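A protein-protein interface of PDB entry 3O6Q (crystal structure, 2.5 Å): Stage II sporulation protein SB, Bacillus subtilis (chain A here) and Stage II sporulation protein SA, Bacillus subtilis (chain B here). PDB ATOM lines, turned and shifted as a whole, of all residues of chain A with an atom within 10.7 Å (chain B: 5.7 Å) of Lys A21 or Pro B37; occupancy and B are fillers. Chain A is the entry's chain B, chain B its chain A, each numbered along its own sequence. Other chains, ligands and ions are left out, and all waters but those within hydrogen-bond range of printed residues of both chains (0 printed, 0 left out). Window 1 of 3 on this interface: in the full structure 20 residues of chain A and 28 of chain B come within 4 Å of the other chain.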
ATOM      1  N   LYS A  18     -14.292  19.478  -4.912  1.00  0.00           N
ATOM      2  CA  LYS A  18     -14.669  18.504  -3.870  1.00  0.00           C
ATOM      3  C   LYS A  18     -13.963  18.808  -2.536  1.00  0.00           C
ATOM      4  O   LYS A  18     -12.829  19.278  -2.520  1.00  0.00           O
ATOM      5  CB  LYS A  18     -14.264  17.078  -4.322  1.00  0.00           C
ATOM      6  CG  LYS A  18     -14.491  16.751  -5.809  1.00  0.00           C
ATOM      7  CD  LYS A  18     -13.460  15.735  -6.385  1.00  0.00           C
ATOM      8  CE  LYS A  18     -13.174  15.952  -7.911  1.00  0.00           C
ATOM      9  NZ  LYS A  18     -11.888  15.354  -8.405  1.00  0.00           N
ATOM     10  N   ILE A  19     -14.635  18.507  -1.429  1.00  0.00           N
ATOM     11  CA  ILE A  19     -14.057  18.614  -0.073  1.00  0.00           C
ATOM     12  C   ILE A  19     -14.390  17.347   0.763  1.00  0.00           C
ATOM     13  O   ILE A  19     -15.557  17.029   0.976  1.00  0.00           O
ATOM     14  CB  ILE A  19     -14.480  19.973   0.631  1.00  0.00           C
ATOM     15  CG1 ILE A  19     -14.912  19.797   2.099  1.00  0.00           C
ATOM     16  CG2 ILE A  19     -15.586  20.672  -0.146  1.00  0.00           C
ATOM     17  CD1 ILE A  19     -15.219  21.123   2.829  1.00  0.00           C
ATOM     18  N   LEU A  20     -13.362  16.628   1.220  1.00  0.00           N
ATOM     19  CA  LEU A  20     -13.541  15.389   1.986  1.00  0.00           C
ATOM     20  C   LEU A  20     -13.503  15.785   3.440  1.00  0.00           C
ATOM     21  O   LEU A  20     -12.530  16.376   3.884  1.00  0.00           O
ATOM     22  CB  LEU A  20     -12.411  14.396   1.677  1.00  0.00           C
ATOM     23  CG  LEU A  20     -12.667  12.889   1.747  1.00  0.00           C
ATOM     24  CD1 LEU A  20     -13.612  12.472   0.649  1.00  0.00           C
ATOM     25  CD2 LEU A  20     -11.343  12.102   1.640  1.00  0.00           C
ATOM     26  N   LYS A  21     -14.573  15.512   4.175  1.00  0.00           N
ATOM     27  CA  LYS A  21     -14.639  15.834   5.600  1.00  0.00           C
ATOM     28  C   LYS A  21     -14.791  14.533   6.396  1.00  0.00           C
ATOM     29  O   LYS A  21     -15.490  13.625   5.958  1.00  0.00           O
ATOM     30  CB  LYS A  21     -15.837  16.761   5.894  1.00  0.00           C
ATOM     31  CG  LYS A  21     -15.701  18.220   5.430  1.00  0.00           C
ATOM     32  CD  LYS A  21     -15.482  19.203   6.594  1.00  0.00           C
ATOM     33  CE  LYS A  21     -15.904  20.634   6.224  1.00  0.00           C
ATOM     34  NZ  LYS A  21     -16.404  21.390   7.400  1.00  0.00           N
ATOM     35  N   LYS A  22     -14.175  14.477   7.576  1.00  0.00           N
ATOM     36  CA  LYS A  22     -14.182  13.274   8.414  1.00  0.00           C
ATOM     37  C   LYS A  22     -14.433  13.530   9.911  1.00  0.00           C
ATOM     38  O   LYS A  22     -13.930  14.490  10.490  1.00  0.00           O
ATOM     39  CB  LYS A  22     -12.875  12.502   8.230  1.00  0.00           C
ATOM     40  CG  LYS A  22     -13.002  11.040   8.691  1.00  0.00           C
ATOM     41  CD  LYS A  22     -11.787  10.180   8.331  1.00  0.00           C
ATOM     42  CE  LYS A  22     -12.101   8.694   8.533  1.00  0.00           C
ATOM     43  NZ  LYS A  22     -10.919   7.862   8.200  1.00  0.00           N
ATOM     44  N   ARG A  23     -15.197  12.644  10.540  1.00  0.00           N
ATOM     45  CA  ARG A  23     -15.417  12.714  11.992  1.00  0.00           C
ATOM     46  C   ARG A  23     -14.159  12.185  12.686  1.00  0.00           C
ATOM     47  O   ARG A  23     -13.920  10.980  12.684  1.00  0.00           O
ATOM     48  CB  ARG A  23     -16.682  11.941  12.391  1.00  0.00           C
ATOM     49  CG  ARG A  23     -16.775  11.419  13.806  1.00  0.00           C
ATOM     50  CD  ARG A  23     -16.310   9.940  13.893  1.00  0.00           C
ATOM     51  NE  ARG A  23     -15.151   9.722  14.754  1.00  0.00           N
ATOM     52  CZ  ARG A  23     -14.510   8.557  14.921  1.00  0.00           C
ATOM     53  NH1 ARG A  23     -14.896   7.447  14.294  1.00  0.00           N
ATOM     54  NH2 ARG A  23     -13.457   8.500  15.736  1.00  0.00           N
ATOM     55  N   SER A  24     -13.361  13.110  13.235  1.00  0.00           N
ATOM     56  CA  SER A  24     -12.012  12.834  13.746  1.00  0.00           C
ATOM     57  C   SER A  24     -11.774  13.272  15.185  1.00  0.00           C
ATOM     58  O   SER A  24     -11.469  12.429  16.043  1.00  0.00           O
ATOM     59  CB  SER A  24     -10.970  13.523  12.870  1.00  0.00           C
ATOM     60  OG  SER A  24     -11.181  14.915  12.805  1.00  0.00           O
ATOM     61  N   THR A  25     -11.896  14.579  15.456  1.00  0.00           N
ATOM     62  CA  THR A  25     -11.632  15.108  16.805  1.00  0.00           C
ATOM     63  C   THR A  25     -12.424  14.410  17.944  1.00  0.00           C
ATOM     64  O   THR A  25     -12.087  14.607  19.122  1.00  0.00           O
ATOM     65  CB  THR A  25     -11.810  16.667  16.895  1.00  0.00           C
ATOM     66  OG1 THR A  25     -13.125  17.052  16.487  1.00  0.00           O
ATOM     67  CG2 THR A  25     -10.783  17.377  16.026  1.00  0.00           C
ATOM     68  N   LEU B  32     -21.696   4.777   9.416  1.00  0.00           N
ATOM     69  CA  LEU B  32     -21.137   5.560   8.297  1.00  0.00           C
ATOM     70  C   LEU B  32     -20.847   7.012   8.684  1.00  0.00           C
ATOM     71  O   LEU B  32     -19.845   7.570   8.310  1.00  0.00           O
ATOM     72  CB  LEU B  32     -22.044   5.506   7.100  1.00  0.00           C
ATOM     73  CG  LEU B  32     -22.237   4.146   6.421  1.00  0.00           C
ATOM     74  CD1 LEU B  32     -23.458   4.255   5.493  1.00  0.00           C
ATOM     75  CD2 LEU B  32     -21.011   3.729   5.638  1.00  0.00           C
ATOM     76  N   ASN B  35     -17.491   6.602  10.471  1.00  0.00           N
ATOM     77  CA  ASN B  35     -16.265   6.073   9.824  1.00  0.00           C
ATOM     78  C   ASN B  35     -16.048   6.452   8.325  1.00  0.00           C
ATOM     79  O   ASN B  35     -14.919   6.393   7.833  1.00  0.00           O
ATOM     80  CB  ASN B  35     -16.234   4.551  10.004  1.00  0.00           C
ATOM     81  CG  ASN B  35     -16.199   4.134  11.498  1.00  0.00           C
ATOM     82  OD1 ASN B  35     -15.254   4.465  12.209  1.00  0.00           O
ATOM     83  ND2 ASN B  35     -17.223   3.427  11.971  1.00  0.00           N
ATOM     84  N   GLU B  36     -17.111   6.852   7.618  1.00  0.00           N
ATOM     85  CA  GLU B  36     -17.025   7.219   6.200  1.00  0.00           C
ATOM     86  C   GLU B  36     -16.930   8.740   5.925  1.00  0.00           C
ATOM     87  O   GLU B  36     -17.818   9.521   6.273  1.00  0.00           O
ATOM     88  CB  GLU B  36     -18.208   6.647   5.418  1.00  0.00           C
ATOM     89  CG  GLU B  36     -18.061   5.183   5.082  1.00  0.00           C
ATOM     90  CD  GLU B  36     -17.250   4.919   3.807  1.00  0.00           C
ATOM     91  OE1 GLU B  36     -17.643   5.419   2.723  1.00  0.00           O
ATOM     92  OE2 GLU B  36     -16.238   4.193   3.897  1.00  0.00           O
ATOM     93  N   PRO B  37     -15.858   9.160   5.246  1.00  0.00           N
ATOM     94  CA  PRO B  37     -15.764  10.583   4.937  1.00  0.00           C
ATOM     95  C   PRO B  37     -16.877  11.012   4.015  1.00  0.00           C
ATOM     96  O   PRO B  37     -17.151  10.317   3.038  1.00  0.00           O
ATOM     97  CB  PRO B  37     -14.416  10.688   4.216  1.00  0.00           C
ATOM     98  CG  PRO B  37     -14.176   9.343   3.674  1.00  0.00           C
ATOM     99  CD  PRO B  37     -14.743   8.395   4.671  1.00  0.00           C
ATOM    100  N   ILE B  38     -17.500  12.151   4.305  1.00  0.00           N
ATOM    101  CA  ILE B  38     -18.397  12.754   3.330  1.00  0.00           C
ATOM    102  C   ILE B  38     -17.581  13.484   2.258  1.00  0.00           C
ATOM    103  O   ILE B  38     -16.654  14.255   2.570  1.00  0.00           O
ATOM    104  CB  ILE B  38     -19.361  13.716   3.960  1.00  0.00           C
ATOM    105  CG1 ILE B  38     -20.191  13.016   5.040  1.00  0.00           C
ATOM    106  CG2 ILE B  38     -20.298  14.222   2.893  1.00  0.00           C
ATOM    107  CD1 ILE B  38     -21.494  13.797   5.431  1.00  0.00           C
ATOM    108  N   HIS B  39     -17.901  13.196   1.001  1.00  0.00           N
ATOM    109  CA  HIS B  39     -17.311  13.868  -0.159  1.00  0.00           C
ATOM    110  C   HIS B  39     -18.237  15.012  -0.591  1.00  0.00           C
ATOM    111  O   HIS B  39     -19.344  14.778  -1.077  1.00  0.00           O
ATOM    112  CB  HIS B  39     -17.168  12.866  -1.301  1.00  0.00           C
ATOM    113  CG  HIS B  39     -16.264  11.709  -0.993  1.00  0.00           C
ATOM    114  ND1 HIS B  39     -15.119  11.446  -1.719  1.00  0.00           N
ATOM    115  CD2 HIS B  39     -16.338  10.739  -0.049  1.00  0.00           C
ATOM    116  CE1 HIS B  39     -14.533  10.361  -1.241  1.00  0.00           C
ATOM    117  NE2 HIS B  39     -15.247   9.918  -0.219  1.00  0.00           N
ATOM    118  N   VAL B  40     -17.792  16.256  -0.421  1.00  0.00           N
ATOM    119  CA  VAL B  40     -18.645  17.436  -0.701  1.00  0.00           C
ATOM    120  C   VAL B  40     -18.316  18.139  -2.016  1.00  0.00           C
ATOM    121  O   VAL B  40     -17.235  18.675  -2.179  1.00  0.00           O
ATOM    122  CB  VAL B  40     -18.577  18.449   0.434  1.00  0.00           C
ATOM    123  CG1 VAL B  40     -19.364  19.673   0.090  1.00  0.00           C
ATOM    124  CG2 VAL B  40     -19.098  17.783   1.723  1.00  0.00           C
ATOM    125  N   VAL B 148     -22.317  20.843   5.996  1.00  0.00           N
ATOM    126  CA  VAL B 148     -20.924  20.575   5.861  1.00  0.00           C
ATOM    127  C   VAL B 148     -20.256  21.528   4.849  1.00  0.00           C
ATOM    128  O   VAL B 148     -19.034  21.665   4.856  1.00  0.00           O
ATOM    129  CB  VAL B 148     -20.716  19.113   5.497  1.00  0.00           C
ATOM    130  CG1 VAL B 148     -19.472  18.952   4.687  1.00  0.00           C
ATOM    131  CG2 VAL B 148     -20.678  18.271   6.775  1.00  0.00           C
ATOM    132  N   PRO B 150     -18.683  24.927   3.197  1.00  0.00           N
ATOM    133  CA  PRO B 150     -18.058  26.119   3.792  1.00  0.00           C
ATOM    134  C   PRO B 150     -18.849  27.387   3.476  1.00  0.00           C
ATOM    135  O   PRO B 150     -19.619  27.851   4.306  1.00  0.00           O
ATOM    136  CB  PRO B 150     -16.666  26.167   3.130  1.00  0.00           C
ATOM    137  CG  PRO B 150     -16.483  24.817   2.462  1.00  0.00           C
ATOM    138  CD  PRO B 150     -17.863  24.366   2.106  1.00  0.00           C
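O of Ile B38 is in hydrogen-bond range of N of Lys A21, 2.9 Å away. The backbone carbonyl oxygen (O) of Val B40 lies within hydrogen-bond range of the backbone NH (N) of Ile A19. The backbone carbonyl oxygen (O) of Ile A19 lies close to the backbone carbonyl oxygen (O) of Ile B38 (3.4 Å).
Among the printed residues, pairs that only touch across the chains: Lys A18 with Val B40 (3.1 Å), Ile A19 with His B39 (3.7 Å), Ile A19 with Pro B150 (3.9 Å), Leu A20 with Pro B37 (3.7 Å), Leu A20 with Ile B38 (3.4 Å), Leu A20 with His B39 (3.0 Å), Lys A21 with Pro B37 (3.2 Å), Lys A21 with Val B148 (3.6 Å), Lys A22 with Asn B35 (3.7 Å) and Arg A23 with Asn B35 (3.7 Å).
Of the printed residues of chain B, Lys A18 touches Val B40 (3.1 Å). Printed residues of chain B within 4 Å of Arg A23: Asn B35. Ser A24 touches none of the printed residues of chain B. Leu B32 touches none of the printed residues of chain A. Of chain A, only Leu A20 (3.7 Å) and Lys A21 (3.2 Å) come within 4 Å of Pro B37. Of chain A, only Ile A19 (3.7 Å) and Leu A20 (3.0 Å) come within 4 Å of His B39. Val B148 touches just one residue of chain A: Lys A21. The nearest residue of chain B that does not touch Lys A21 is Glu B36 (4.7 Å). The nearest residue of chain A that does not touch Pro B37 is Lys A22 (4.7 Å). The nearest printed residue of chain A that does not touch Val B40 is Leu A20 (4.7 Å).
Hydrophobic or aromatic side chains of chain A that line the printed part of chain B: Ile A19 and Leu A20. Hydrophobic or aromatic side chains of chain B that line the printed part of chain A: Pro B37, His B39, Val B40, Val B148 and Pro B150. Among the printed residues, no Asp or Glu carboxylate lies within 4 Å of a Lys or Arg side-chain nitrogen of the other chain.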
